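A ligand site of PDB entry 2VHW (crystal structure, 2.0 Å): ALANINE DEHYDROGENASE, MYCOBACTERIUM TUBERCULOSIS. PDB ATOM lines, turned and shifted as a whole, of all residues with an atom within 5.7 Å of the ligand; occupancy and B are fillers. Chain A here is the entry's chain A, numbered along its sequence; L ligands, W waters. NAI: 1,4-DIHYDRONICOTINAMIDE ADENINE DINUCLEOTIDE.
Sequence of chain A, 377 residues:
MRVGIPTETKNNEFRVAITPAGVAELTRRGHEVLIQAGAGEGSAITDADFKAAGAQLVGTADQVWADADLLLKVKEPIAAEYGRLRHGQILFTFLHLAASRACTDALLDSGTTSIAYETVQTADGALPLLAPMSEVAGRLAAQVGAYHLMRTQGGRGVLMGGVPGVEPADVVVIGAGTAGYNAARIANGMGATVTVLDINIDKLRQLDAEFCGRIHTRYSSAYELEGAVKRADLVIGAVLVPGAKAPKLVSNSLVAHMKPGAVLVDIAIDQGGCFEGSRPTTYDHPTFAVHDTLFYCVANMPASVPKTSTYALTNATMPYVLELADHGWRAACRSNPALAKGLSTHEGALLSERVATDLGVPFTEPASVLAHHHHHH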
ATOM      1  N   LEU A 130      -9.045 -27.265 -12.124  1.00  0.00           N
ATOM      2  CA  LEU A 130      -7.910 -26.544 -11.555  1.00  0.00           C
ATOM      3  C   LEU A 130      -6.606 -27.041 -12.179  1.00  0.00           C
ATOM      4  O   LEU A 130      -5.681 -26.264 -12.372  1.00  0.00           O
ATOM      5  CB  LEU A 130      -7.865 -26.678 -10.022  1.00  0.00           C
ATOM      6  CG  LEU A 130      -6.494 -26.373  -9.391  1.00  0.00           C
ATOM      7  CD1 LEU A 130      -6.074 -24.878  -9.504  1.00  0.00           C
ATOM      8  CD2 LEU A 130      -6.350 -26.870  -7.952  1.00  0.00           C
ATOM      9  N   ALA A 131      -6.538 -28.340 -12.500  1.00  0.00           N
ATOM     10  CA  ALA A 131      -5.315 -28.943 -13.052  1.00  0.00           C
ATOM     11  C   ALA A 131      -4.590 -28.135 -14.129  1.00  0.00           C
ATOM     12  O   ALA A 131      -3.393 -27.866 -13.995  1.00  0.00           O
ATOM     13  CB  ALA A 131      -5.554 -30.400 -13.502  1.00  0.00           C
ATOM     14  N   MET A 133      -4.641 -25.004 -14.776  1.00  0.00           N
ATOM     15  CA  MET A 133      -4.143 -23.737 -14.254  1.00  0.00           C
ATOM     16  C   MET A 133      -2.929 -23.937 -13.351  1.00  0.00           C
ATOM     17  O   MET A 133      -2.069 -23.079 -13.281  1.00  0.00           O
ATOM     18  CB  MET A 133      -5.246 -22.964 -13.526  1.00  0.00           C
ATOM     19  CG  MET A 133      -6.490 -22.604 -14.373  1.00  0.00           C
ATOM     20  SD  MET A 133      -6.168 -21.511 -15.772  1.00  0.00           S
ATOM     21  CE  MET A 133      -5.722 -22.698 -17.049  1.00  0.00           C
ATOM     22  N   SER A 134      -2.861 -25.097 -12.691  1.00  0.00           N
ATOM     23  CA  SER A 134      -1.652 -25.488 -11.967  1.00  0.00           C
ATOM     24  C   SER A 134      -0.486 -25.787 -12.909  1.00  0.00           C
ATOM     25  O   SER A 134       0.663 -25.440 -12.611  1.00  0.00           O
ATOM     26  CB  SER A 134      -1.959 -26.685 -11.070  1.00  0.00           C
ATOM     27  OG  SER A 134      -2.836 -26.318 -10.024  1.00  0.00           O
ATOM     28  N   ALA A 137       0.719 -22.286 -14.138  1.00  0.00           N
ATOM     29  CA  ALA A 137       1.398 -21.612 -13.034  1.00  0.00           C
ATOM     30  C   ALA A 137       2.787 -22.216 -12.752  1.00  0.00           C
ATOM     31  O   ALA A 137       3.742 -21.472 -12.579  1.00  0.00           O
ATOM     32  CB  ALA A 137       0.525 -21.610 -11.756  1.00  0.00           C
ATOM     33  N   ILE A 174       9.094 -26.892  -3.716  1.00  0.00           N
ATOM     34  CA  ILE A 174       8.412 -27.497  -2.544  1.00  0.00           C
ATOM     35  C   ILE A 174       7.033 -27.918  -3.013  1.00  0.00           C
ATOM     36  O   ILE A 174       6.186 -27.043  -3.322  1.00  0.00           O
ATOM     37  CB  ILE A 174       8.253 -26.464  -1.404  1.00  0.00           C
ATOM     38  CG1 ILE A 174       9.598 -25.745  -1.155  1.00  0.00           C
ATOM     39  CG2 ILE A 174       7.680 -27.149  -0.134  1.00  0.00           C
ATOM     40  CD1 ILE A 174       9.506 -24.671  -0.050  1.00  0.00           C
ATOM     41  N   GLY A 175       6.813 -29.219  -3.096  1.00  0.00           N
ATOM     42  CA  GLY A 175       5.606 -29.790  -3.710  1.00  0.00           C
ATOM     43  C   GLY A 175       5.879 -30.435  -5.063  1.00  0.00           C
ATOM     44  O   GLY A 175       6.355 -29.746  -5.966  1.00  0.00           O
ATOM     45  N   ALA A 176       5.510 -31.715  -5.214  1.00  0.00           N
ATOM     46  CA  ALA A 176       5.730 -32.510  -6.428  1.00  0.00           C
ATOM     47  C   ALA A 176       4.389 -32.831  -7.133  1.00  0.00           C
ATOM     48  O   ALA A 176       4.259 -33.834  -7.818  1.00  0.00           O
ATOM     49  CB  ALA A 176       6.520 -33.814  -6.107  1.00  0.00           C
ATOM     50  N   GLY A 177       3.389 -31.973  -6.945  1.00  0.00           N
ATOM     51  CA  GLY A 177       2.087 -32.227  -7.547  1.00  0.00           C
ATOM     52  C   GLY A 177       2.052 -31.544  -8.906  1.00  0.00           C
ATOM     53  O   GLY A 177       3.092 -31.407  -9.554  1.00  0.00           O
ATOM     54  N   THR A 178       0.867 -31.102  -9.325  1.00  0.00           N
ATOM     55  CA  THR A 178       0.719 -30.586 -10.703  1.00  0.00           C
ATOM     56  C   THR A 178       1.619 -29.385 -10.969  1.00  0.00           C
ATOM     57  O   THR A 178       2.413 -29.400 -11.907  1.00  0.00           O
ATOM     58  CB  THR A 178      -0.760 -30.286 -11.053  1.00  0.00           C
ATOM     59  OG1 THR A 178      -1.529 -31.469 -10.858  1.00  0.00           O
ATOM     60  CG2 THR A 178      -0.883 -29.871 -12.489  1.00  0.00           C
ATOM     61  N   ALA A 179       1.529 -28.361 -10.122  1.00  0.00           N
ATOM     62  CA  ALA A 179       2.339 -27.163 -10.328  1.00  0.00           C
ATOM     63  C   ALA A 179       3.812 -27.407 -10.061  1.00  0.00           C
ATOM     64  O   ALA A 179       4.668 -26.975 -10.833  1.00  0.00           O
ATOM     65  CB  ALA A 179       1.795 -25.964  -9.487  1.00  0.00           C
ATOM     66  N   GLY A 180       4.104 -28.139  -8.980  1.00  0.00           N
ATOM     67  CA  GLY A 180       5.472 -28.464  -8.617  1.00  0.00           C
ATOM     68  C   GLY A 180       6.223 -29.226  -9.679  1.00  0.00           C
ATOM     69  O   GLY A 180       7.336 -28.845 -10.027  1.00  0.00           O
ATOM     70  N   LEU A 197      10.879 -31.440  -3.249  1.00  0.00           N
ATOM     71  CA  LEU A 197      10.502 -32.037  -1.960  1.00  0.00           C
ATOM     72  C   LEU A 197       9.016 -32.304  -1.907  1.00  0.00           C
ATOM     73  O   LEU A 197       8.208 -31.480  -2.321  1.00  0.00           O
ATOM     74  CB  LEU A 197      10.927 -31.124  -0.791  1.00  0.00           C
ATOM     75  CG  LEU A 197      12.455 -31.004  -0.640  1.00  0.00           C
ATOM     76  CD1 LEU A 197      12.974 -29.714  -1.246  1.00  0.00           C
ATOM     77  CD2 LEU A 197      12.872 -31.117   0.810  1.00  0.00           C
ATOM     78  N   ASP A 198       8.668 -33.494  -1.413  1.00  0.00           N
ATOM     79  CA  ASP A 198       7.276 -33.832  -1.132  1.00  0.00           C
ATOM     80  C   ASP A 198       7.215 -34.819   0.034  1.00  0.00           C
ATOM     81  O   ASP A 198       8.193 -35.548   0.305  1.00  0.00           O
ATOM     82  CB  ASP A 198       6.576 -34.431  -2.364  1.00  0.00           C
ATOM     83  CG  ASP A 198       5.058 -34.143  -2.383  1.00  0.00           C
ATOM     84  OD1 ASP A 198       4.361 -34.539  -1.448  1.00  0.00           O
ATOM     85  OD2 ASP A 198       4.575 -33.523  -3.338  1.00  0.00           O
ATOM     86  N   ILE A 199       6.077 -34.848   0.711  1.00  0.00           N
ATOM     87  CA  ILE A 199       5.798 -35.870   1.740  1.00  0.00           C
ATOM     88  C   ILE A 199       5.251 -37.143   1.082  1.00  0.00           C
ATOM     89  O   ILE A 199       5.292 -38.232   1.695  1.00  0.00           O
ATOM     90  CB  ILE A 199       4.789 -35.324   2.797  1.00  0.00           C
ATOM     91  CG1 ILE A 199       3.536 -34.777   2.094  1.00  0.00           C
ATOM     92  CG2 ILE A 199       5.472 -34.226   3.619  1.00  0.00           C
ATOM     93  CD1 ILE A 199       2.354 -34.403   3.034  1.00  0.00           C
ATOM     94  N   ASN A 200       4.757 -37.015  -0.160  1.00  0.00           N
ATOM     95  CA  ASN A 200       4.272 -38.155  -0.945  1.00  0.00           C
ATOM     96  C   ASN A 200       5.426 -38.805  -1.731  1.00  0.00           C
ATOM     97  O   ASN A 200       5.846 -38.286  -2.773  1.00  0.00           O
ATOM     98  CB  ASN A 200       3.159 -37.724  -1.913  1.00  0.00           C
ATOM     99  CG  ASN A 200       2.480 -38.909  -2.602  1.00  0.00           C
ATOM    100  OD1 ASN A 200       3.094 -39.958  -2.857  1.00  0.00           O
ATOM    101  ND2 ASN A 200       1.189 -38.752  -2.887  1.00  0.00           N
ATOM    102  N   LYS A 203       5.103 -39.704  -5.552  1.00  0.00           N
ATOM    103  CA  LYS A 203       5.367 -38.586  -6.449  1.00  0.00           C
ATOM    104  C   LYS A 203       6.866 -38.339  -6.694  1.00  0.00           C
ATOM    105  O   LYS A 203       7.262 -37.920  -7.796  1.00  0.00           O
ATOM    106  CB  LYS A 203       4.658 -37.333  -5.957  1.00  0.00           C
ATOM    107  CG  LYS A 203       3.149 -37.504  -6.136  1.00  0.00           C
ATOM    108  CD  LYS A 203       2.405 -36.257  -5.837  1.00  0.00           C
ATOM    109  CE  LYS A 203       0.886 -36.453  -6.050  1.00  0.00           C
ATOM    110  NZ  LYS A 203       0.168 -35.200  -5.673  1.00  0.00           N
ATOM    111  N   SER A 220      10.235 -34.598   2.202  1.00  0.00           N
ATOM    112  CA  SER A 220      10.001 -33.307   2.801  1.00  0.00           C
ATOM    113  C   SER A 220       9.898 -33.424   4.319  1.00  0.00           C
ATOM    114  O   SER A 220       9.030 -34.135   4.847  1.00  0.00           O
ATOM    115  CB  SER A 220       8.740 -32.681   2.253  1.00  0.00           C
ATOM    116  OG  SER A 220       8.773 -31.309   2.517  1.00  0.00           O
ATOM    117  N   LEU A 225      14.080 -29.456   4.438  1.00  0.00           N
ATOM    118  CA  LEU A 225      13.615 -28.265   3.763  1.00  0.00           C
ATOM    119  C   LEU A 225      14.514 -27.077   4.126  1.00  0.00           C
ATOM    120  O   LEU A 225      14.928 -26.330   3.249  1.00  0.00           O
ATOM    121  CB  LEU A 225      12.164 -28.018   4.141  1.00  0.00           C
ATOM    122  CG  LEU A 225      11.227 -27.150   3.315  1.00  0.00           C
ATOM    123  CD1 LEU A 225       9.827 -27.723   3.456  1.00  0.00           C
ATOM    124  CD2 LEU A 225      11.262 -25.744   3.869  1.00  0.00           C
ATOM    125  N   ALA A 238       5.011 -24.776  -4.084  1.00  0.00           N
ATOM    126  CA  ALA A 238       3.919 -25.383  -4.897  1.00  0.00           C
ATOM    127  C   ALA A 238       3.059 -26.418  -4.125  1.00  0.00           C
ATOM    128  O   ALA A 238       2.587 -27.415  -4.677  1.00  0.00           O
ATOM    129  CB  ALA A 238       4.499 -25.990  -6.174  1.00  0.00           C
ATOM    130  N   VAL A 239       2.827 -26.112  -2.859  1.00  0.00           N
ATOM    131  CA  VAL A 239       2.173 -27.016  -1.931  1.00  0.00           C
ATOM    132  C   VAL A 239       0.625 -26.827  -1.897  1.00  0.00           C
ATOM    133  O   VAL A 239       0.116 -25.722  -2.058  1.00  0.00           O
ATOM    134  CB  VAL A 239       2.837 -26.858  -0.539  1.00  0.00           C
ATOM    135  CG1 VAL A 239       1.977 -27.359   0.591  1.00  0.00           C
ATOM    136  CG2 VAL A 239       4.194 -27.541  -0.545  1.00  0.00           C
ATOM    137  N   LEU A 240      -0.101 -27.955  -1.773  1.00  0.00           N
ATOM    138  CA  LEU A 240      -1.537 -27.956  -1.488  1.00  0.00           C
ATOM    139  C   LEU A 240      -1.884 -29.094  -0.508  1.00  0.00           C
ATOM    140  O   LEU A 240      -1.563 -30.268  -0.745  1.00  0.00           O
ATOM    141  CB  LEU A 240      -2.379 -28.084  -2.768  1.00  0.00           C
ATOM    142  CG  LEU A 240      -3.889 -28.330  -2.629  1.00  0.00           C
ATOM    143  CD1 LEU A 240      -4.618 -27.072  -2.173  1.00  0.00           C
ATOM    144  CD2 LEU A 240      -4.509 -28.846  -3.922  1.00  0.00           C
ATOM    145  N   VAL A 241      -2.523 -28.713   0.607  1.00  0.00           N
ATOM    146  CA  VAL A 241      -3.081 -29.657   1.568  1.00  0.00           C
ATOM    147  C   VAL A 241      -4.589 -29.611   1.362  1.00  0.00           C
ATOM    148  O   VAL A 241      -5.194 -28.570   1.609  1.00  0.00           O
ATOM    149  CB  VAL A 241      -2.713 -29.274   3.034  1.00  0.00           C
ATOM    150  CG1 VAL A 241      -3.388 -30.194   4.039  1.00  0.00           C
ATOM    151  CG2 VAL A 241      -1.188 -29.272   3.235  1.00  0.00           C
ATOM    152  N   PRO A 247       0.309 -24.510   4.433  1.00  0.00           N
ATOM    153  CA  PRO A 247       1.179 -24.475   5.616  1.00  0.00           C
ATOM    154  C   PRO A 247       2.349 -23.527   5.362  1.00  0.00           C
ATOM    155  O   PRO A 247       2.802 -23.417   4.218  1.00  0.00           O
ATOM    156  CB  PRO A 247       1.679 -25.921   5.750  1.00  0.00           C
ATOM    157  CG  PRO A 247       1.572 -26.489   4.376  1.00  0.00           C
ATOM    158  CD  PRO A 247       0.367 -25.824   3.749  1.00  0.00           C
ATOM    159  N   LEU A 249       5.735 -23.172   5.428  1.00  0.00           N
ATOM    160  CA  LEU A 249       6.844 -24.101   5.410  1.00  0.00           C
ATOM    161  C   LEU A 249       8.191 -23.391   5.433  1.00  0.00           C
ATOM    162  O   LEU A 249       9.189 -23.969   5.887  1.00  0.00           O
ATOM    163  CB  LEU A 249       6.739 -24.977   4.167  1.00  0.00           C
ATOM    164  CG  LEU A 249       6.089 -26.377   4.172  1.00  0.00           C
ATOM    165  CD1 LEU A 249       5.358 -26.756   5.439  1.00  0.00           C
ATOM    166  CD2 LEU A 249       5.167 -26.502   2.954  1.00  0.00           C
ATOM    167  N   ASP A 266       6.017 -17.887  -4.737  1.00  0.00           N
ATOM    168  CA  ASP A 266       4.989 -18.612  -3.991  1.00  0.00           C
ATOM    169  C   ASP A 266       3.768 -18.792  -4.871  1.00  0.00           C
ATOM    170  O   ASP A 266       2.909 -17.900  -4.936  1.00  0.00           O
ATOM    171  CB  ASP A 266       4.594 -17.833  -2.738  1.00  0.00           C
ATOM    172  CG  ASP A 266       3.963 -18.708  -1.639  1.00  0.00           C
ATOM    173  OD1 ASP A 266       3.549 -19.870  -1.850  1.00  0.00           O
ATOM    174  OD2 ASP A 266       3.900 -18.185  -0.514  1.00  0.00           O
ATOM    175  N   ILE A 267       3.682 -19.947  -5.547  1.00  0.00           N
ATOM    176  CA  ILE A 267       2.507 -20.299  -6.316  1.00  0.00           C
ATOM    177  C   ILE A 267       1.285 -20.420  -5.392  1.00  0.00           C
ATOM    178  O   ILE A 267       0.185 -20.038  -5.782  1.00  0.00           O
ATOM    179  CB  ILE A 267       2.692 -21.606  -7.123  1.00  0.00           C
ATOM    180  CG1 ILE A 267       4.004 -21.576  -7.942  1.00  0.00           C
ATOM    181  CG2 ILE A 267       1.491 -21.860  -8.020  1.00  0.00           C
ATOM    182  CD1 ILE A 267       4.178 -22.730  -8.895  1.00  0.00           C
ATOM    183  N   ALA A 268       1.508 -20.934  -4.171  1.00  0.00           N
ATOM    184  CA  ALA A 268       0.420 -21.202  -3.206  1.00  0.00           C
ATOM    185  C   ALA A 268      -0.158 -19.944  -2.548  1.00  0.00           C
ATOM    186  O   ALA A 268      -0.947 -20.017  -1.579  1.00  0.00           O
ATOM    187  CB  ALA A 268       0.856 -22.221  -2.166  1.00  0.00           C
ATOM    188  N   ILE A 269       0.197 -18.781  -3.093  1.00  0.00           N
ATOM    189  CA  ILE A 269      -0.323 -17.500  -2.626  1.00  0.00           C
ATOM    190  C   ILE A 269      -1.861 -17.407  -2.705  1.00  0.00           C
ATOM    191  O   ILE A 269      -2.486 -16.603  -2.003  1.00  0.00           O
ATOM    192  CB  ILE A 269       0.373 -16.304  -3.364  1.00  0.00           C
ATOM    193  CG1 ILE A 269       0.091 -14.969  -2.652  1.00  0.00           C
ATOM    194  CG2 ILE A 269       0.002 -16.299  -4.836  1.00  0.00           C
ATOM    195  CD1 ILE A 269       0.434 -14.979  -1.157  1.00  0.00           C
ATOM    196  N   ASP A 270      -2.469 -18.237  -3.546  1.00  0.00           N
ATOM    197  CA  ASP A 270      -3.927 -18.241  -3.658  1.00  0.00           C
ATOM    198  C   ASP A 270      -4.628 -18.860  -2.418  1.00  0.00           C
ATOM    199  O   ASP A 270      -5.850 -18.898  -2.370  1.00  0.00           O
ATOM    200  CB  ASP A 270      -4.380 -18.882  -4.994  1.00  0.00           C
ATOM    201  CG  ASP A 270      -4.018 -20.363  -5.112  1.00  0.00           C
ATOM    202  OD1 ASP A 270      -4.611 -21.020  -6.009  1.00  0.00           O
ATOM    203  OD2 ASP A 270      -3.153 -20.877  -4.370  1.00  0.00           O
ATOM    204  N   GLN A 271      -3.828 -19.270  -1.424  1.00  0.00           N
ATOM    205  CA  GLN A 271      -4.311 -19.939  -0.203  1.00  0.00           C
ATOM    206  C   GLN A 271      -3.455 -19.777   1.071  1.00  0.00           C
ATOM    207  O   GLN A 271      -3.656 -20.514   2.021  1.00  0.00           O
ATOM    208  CB  GLN A 271      -4.285 -21.474  -0.435  1.00  0.00           C
ATOM    209  CG  GLN A 271      -4.930 -22.015  -1.703  1.00  0.00           C
ATOM    210  CD  GLN A 271      -6.122 -22.875  -1.412  1.00  0.00           C
ATOM    211  OE1 GLN A 271      -7.226 -22.387  -1.100  1.00  0.00           O
ATOM    212  NE2 GLN A 271      -5.922 -24.181  -1.494  1.00  0.00           N
ATOM    213  N   VAL A 298       2.209 -13.744  -7.140  1.00  0.00           N
ATOM    214  CA  VAL A 298       0.998 -13.354  -7.855  1.00  0.00           C
ATOM    215  C   VAL A 298      -0.057 -14.472  -7.863  1.00  0.00           C
ATOM    216  O   VAL A 298       0.261 -15.651  -8.121  1.00  0.00           O
ATOM    217  CB  VAL A 298       1.237 -12.608  -9.227  1.00  0.00           C
ATOM    218  CG1 VAL A 298       2.672 -12.073  -9.299  1.00  0.00           C
ATOM    219  CG2 VAL A 298       0.903 -13.463 -10.424  1.00  0.00           C
ATOM    220  N   ALA A 299      -1.284 -14.078  -7.541  1.00  0.00           N
ATOM    221  CA  ALA A 299      -2.363 -15.026  -7.295  1.00  0.00           C
ATOM    222  C   ALA A 299      -3.112 -15.385  -8.577  1.00  0.00           C
ATOM    223  O   ALA A 299      -3.893 -16.339  -8.587  1.00  0.00           O
ATOM    224  CB  ALA A 299      -3.324 -14.473  -6.247  1.00  0.00           C
ATOM    225  N   ASN A 300      -2.856 -14.629  -9.646  1.00  0.00           N
ATOM    226  CA  ASN A 300      -3.448 -14.896 -10.960  1.00  0.00           C
ATOM    227  C   ASN A 300      -2.383 -15.150 -12.030  1.00  0.00           C
ATOM    228  O   ASN A 300      -2.397 -14.529 -13.095  1.00  0.00           O
ATOM    229  CB  ASN A 300      -4.397 -13.741 -11.372  1.00  0.00           C
ATOM    230  CG  ASN A 300      -5.818 -13.929 -10.860  1.00  0.00           C
ATOM    231  OD1 ASN A 300      -6.148 -14.917 -10.173  1.00  0.00           O
ATOM    232  ND2 ASN A 300      -6.690 -12.977 -11.195  1.00  0.00           N
ATOM    233  N   MET A 301      -1.474 -16.084 -11.747  1.00  0.00           N
ATOM    234  CA  MET A 301      -0.356 -16.362 -12.660  1.00  0.00           C
ATOM    235  C   MET A 301      -0.818 -16.681 -14.087  1.00  0.00           C
ATOM    236  O   MET A 301      -0.270 -16.117 -15.015  1.00  0.00           O
ATOM    237  CB  MET A 301       0.587 -17.438 -12.103  1.00  0.00           C
ATOM    238  CG  MET A 301       1.438 -16.946 -10.960  1.00  0.00           C
ATOM    239  SD  MET A 301       2.513 -18.183 -10.218  1.00  0.00           S
ATOM    240  CE  MET A 301       4.007 -17.962 -11.155  1.00  0.00           C
ATOM    241  N   PRO A 302      -1.801 -17.592 -14.269  1.00  0.00           N
ATOM    242  CA  PRO A 302      -2.262 -17.900 -15.634  1.00  0.00           C
ATOM    243  C   PRO A 302      -2.785 -16.740 -16.487  1.00  0.00           C
ATOM    244  O   PRO A 302      -2.710 -16.829 -17.706  1.00  0.00           O
ATOM    245  CB  PRO A 302      -3.370 -18.929 -15.386  1.00  0.00           C
ATOM    246  CG  PRO A 302      -2.979 -19.566 -14.124  1.00  0.00           C
ATOM    247  CD  PRO A 302      -2.527 -18.430 -13.296  1.00  0.00           C
HETATM  248  PA  NAI L   1      -1.459 -30.781  -6.093  1.00  0.00           P
HETATM  249  O1A NAI L   1      -2.477 -31.313  -5.095  1.00  0.00           O
HETATM  250  O2A NAI L   1      -1.421 -31.430  -7.452  1.00  0.00           O
HETATM  251  O5B NAI L   1      -0.020 -30.934  -5.411  1.00  0.00           O
HETATM  252  C5B NAI L   1       0.312 -30.340  -4.157  1.00  0.00           C
HETATM  253  C4B NAI L   1       1.424 -31.182  -3.545  1.00  0.00           C
HETATM  254  O4B NAI L   1       1.885 -30.525  -2.382  1.00  0.00           O
HETATM  255  C3B NAI L   1       1.016 -32.595  -3.120  1.00  0.00           C
HETATM  256  O3B NAI L   1       1.702 -33.599  -3.882  1.00  0.00           O
HETATM  257  C2B NAI L   1       1.349 -32.638  -1.638  1.00  0.00           C
HETATM  258  O2B NAI L   1       1.808 -33.878  -1.099  1.00  0.00           O
HETATM  259  C1B NAI L   1       2.393 -31.552  -1.550  1.00  0.00           C
HETATM  260  N9A NAI L   1       2.625 -31.165  -0.159  1.00  0.00           N
HETATM  261  C8A NAI L   1       1.699 -31.015   0.810  1.00  0.00           C
HETATM  262  N7A NAI L   1       2.315 -30.693   1.976  1.00  0.00           N
HETATM  263  C5A NAI L   1       3.651 -30.651   1.770  1.00  0.00           C
HETATM  264  C6A NAI L   1       4.894 -30.397   2.553  1.00  0.00           C
HETATM  265  N6A NAI L   1       4.847 -30.080   3.854  1.00  0.00           N
HETATM  266  N1A NAI L   1       6.086 -30.459   1.919  1.00  0.00           N
HETATM  267  C2A NAI L   1       6.172 -30.760   0.618  1.00  0.00           C
HETATM  268  N3A NAI L   1       5.104 -31.023  -0.133  1.00  0.00           N
HETATM  269  C4A NAI L   1       3.847 -30.979   0.361  1.00  0.00           C
HETATM  270  O3  NAI L   1      -1.628 -29.187  -6.112  1.00  0.00           O
HETATM  271  PN  NAI L   1      -1.304 -28.190  -7.346  1.00  0.00           P
HETATM  272  O1N NAI L   1      -2.395 -28.277  -8.358  1.00  0.00           O
HETATM  273  O2N NAI L   1       0.138 -28.498  -7.758  1.00  0.00           O
HETATM  274  O5D NAI L   1      -1.380 -26.774  -6.634  1.00  0.00           O
HETATM  275  C5D NAI L   1      -0.448 -26.233  -5.696  1.00  0.00           C
HETATM  276  C4D NAI L   1      -0.940 -24.828  -5.344  1.00  0.00           C
HETATM  277  O4D NAI L   1      -0.829 -23.937  -6.478  1.00  0.00           O
HETATM  278  C3D NAI L   1      -2.433 -24.818  -4.970  1.00  0.00           C
HETATM  279  O3D NAI L   1      -2.588 -24.076  -3.762  1.00  0.00           O
HETATM  280  C2D NAI L   1      -3.104 -24.112  -6.124  1.00  0.00           C
HETATM  281  O2D NAI L   1      -4.357 -23.523  -5.765  1.00  0.00           O
HETATM  282  C1D NAI L   1      -2.015 -23.121  -6.532  1.00  0.00           C
HETATM  283  N1N NAI L   1      -2.208 -22.465  -7.837  1.00  0.00           N
HETATM  284  C2N NAI L   1      -1.896 -21.163  -7.917  1.00  0.00           C
HETATM  285  C3N NAI L   1      -2.054 -20.462  -9.089  1.00  0.00           C
HETATM  286  C7N NAI L   1      -1.637 -19.021  -9.141  1.00  0.00           C
HETATM  287  O7N NAI L   1      -1.927 -18.359 -10.130  1.00  0.00           O
HETATM  288  N7N NAI L   1      -0.919 -18.520  -8.143  1.00  0.00           N
HETATM  289  C4N NAI L   1      -2.531 -21.111 -10.215  1.00  0.00           C
HETATM  290  C5N NAI L   1      -2.838 -22.458 -10.124  1.00  0.00           C
HETATM  291  C6N NAI L   1      -2.659 -23.113  -8.915  1.00  0.00           C
HETATM  292  O   HOH W   1       2.020 -30.990   4.999  1.00  0.00           O
HETATM  293  O   HOH W   2       0.224 -35.912  -2.940  1.00  0.00           O
HETATM  294  O   HOH W   3       2.594 -29.070  -6.708  1.00  0.00           O
HETATM  295  O   HOH W   4      -4.769 -18.288 -10.571  1.00  0.00           O
HETATM  296  O   HOH W   5      -2.087 -24.330  -1.304  1.00  0.00           O
HETATM  297  O   HOH W   6      -1.340 -34.039  -8.150  1.00  0.00           O
HETATM  298  O   HOH W   7      -2.583 -32.404  -2.427  1.00  0.00           O
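The side-chain carboxylate (OD1) of Asp 198 lies within hydrogen-bond range of the backbone NH (N) of Asn 200 (2.8 Å).
The backbone NH of Ala 176 sits at hydrogen-bond distance from the side-chain carboxylate of Asp 198.
The backbone carbonyl oxygen of Asp 198 is in hydrogen-bond range of the backbone NH of Ser 220, 2.9 Å away.
The side-chain amide oxygen (OD1) of Asn 200 is in hydrogen-bond range of the backbone NH (N) of Lys 203.
The backbone NH (N) of Ala 238 lies within hydrogen-bond range of the backbone carbonyl oxygen (O) of Ile 174, at 2.7 Å.
The backbone carbonyl oxygen (O) of Leu 197 lies within hydrogen-bond range of the backbone NH (N) of Gly 175, 2.8 Å away.
The backbone carbonyl oxygen (O) of Ala 299 sits close to an oxygen (O7N) of the ligand, at 3.2 Å.
Merely in contact with the ligand: Pro 302 (3.2 Å), Gly 177 (3.3 Å), Met 133 (3.3 Å), Ala 238 (3.4 Å), Ala 137 (3.5 Å), Val 239 (3.5 Å), Leu 197 (3.6 Å), Leu 249 (3.7 Å), Gln 271 (3.7 Å), Ile 199 (3.7 Å), Asn 300 (3.8 Å), Gly 175 (3.8 Å), Leu 130 (3.9 Å), Val 241 (3.98 Å) and Ile 174 (3.98 Å).
Hydrophobic or aromatic side chains that line the ligand: Leu 130, Ala 137, Ile 174, Ala 179, Ile 199, Val 239, Leu 240, Val 241, Leu 249, Ile 267, Met 301 and Pro 302.
27 residues have an atom within 4 Å of the ligand: Leu 130, Met 133, Ser 134, Ala 137, Ile 174, Gly 175, Gly 177, Thr 178, Ala 179, Leu 197, Asp 198, Ile 199, Lys 203, Ser 220, Ala 238, Val 239, Leu 240, Val 241, Leu 249, Ile 267, Asp 270, Gln 271, Val 298, Ala 299, Asn 300, Met 301 and Pro 302.
The nearest printed residue that does not touch the ligand is Ile 269 (4.1 Å).
Water W5 bridges an oxygen (O3D) of the ligand (2.5 Å) and the backbone carbonyl oxygen of Val 239 (2.7 Å).
Water W6 bridges O2A of the ligand (2.7 Å) and NZ of Lys 203 (3.1 Å).
Water W3 lies within hydrogen-bond range of the backbone carbonyl oxygen of Ala 238 (2.6 Å), an oxygen (O2N) of the ligand (2.7 Å), the backbone NH of Gly 180 (2.9 Å) and the backbone NH of Gly 177 (3.0 Å).
Water W4 bridges an oxygen (O7N) of the ligand (2.9 Å) and the backbone carbonyl oxygen (O) of Ala 299 (2.9 Å).
Water W7 bridges O1A of the ligand (2.9 Å) and O of Leu 240 (2.9 Å).
Water W2 lies within hydrogen-bond range of the side-chain amino group of Lys 203, an oxygen (O3B) of the ligand and the side-chain amide nitrogen of Asn 200.
The backbone NH (N) of Thr 178 is in hydrogen-bond range of an oxygen (O2A) of the ligand (3.0 Å).
An oxygen (O1N) of the ligand sits at hydrogen-bond distance from the side-chain hydroxyl (OG) of Ser 134.
OG1 of Thr 178 sits at hydrogen-bond distance from O2A of the ligand, at 3.4 Å.
An oxygen (O4B) of the ligand is in hydrogen-bond range of the backbone NH (N) of Leu 240 (3.3 Å).
OD1 of Asp 270 sits at hydrogen-bond distance from O2D of the ligand (2.5 Å).
N7N of the ligand lies within hydrogen-bond range of O of Val 298, 3.1 Å away.
The side-chain carboxylate of Asp 198 sits at hydrogen-bond distance from an oxygen (O2B) of the ligand, at 2.7 Å.
The backbone NH (N) of Ala 179 is in hydrogen-bond range of an oxygen (O2N) of the ligand, 2.7 Å away.
The side-chain hydroxyl (OG) of Ser 220 is in hydrogen-bond range of a nitrogen (N1A) of the ligand, 2.9 Å away.
An oxygen (O7N) of the ligand lies within hydrogen-bond range of the backbone NH of Met 301, at 2.8 Å.
The side-chain amino group (NZ) of Lys 203 sits at hydrogen-bond distance from an oxygen (O3B) of the ligand.
The backbone carbonyl oxygen of Ile 267 is in hydrogen-bond range of a nitrogen (N7N) of the ligand.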
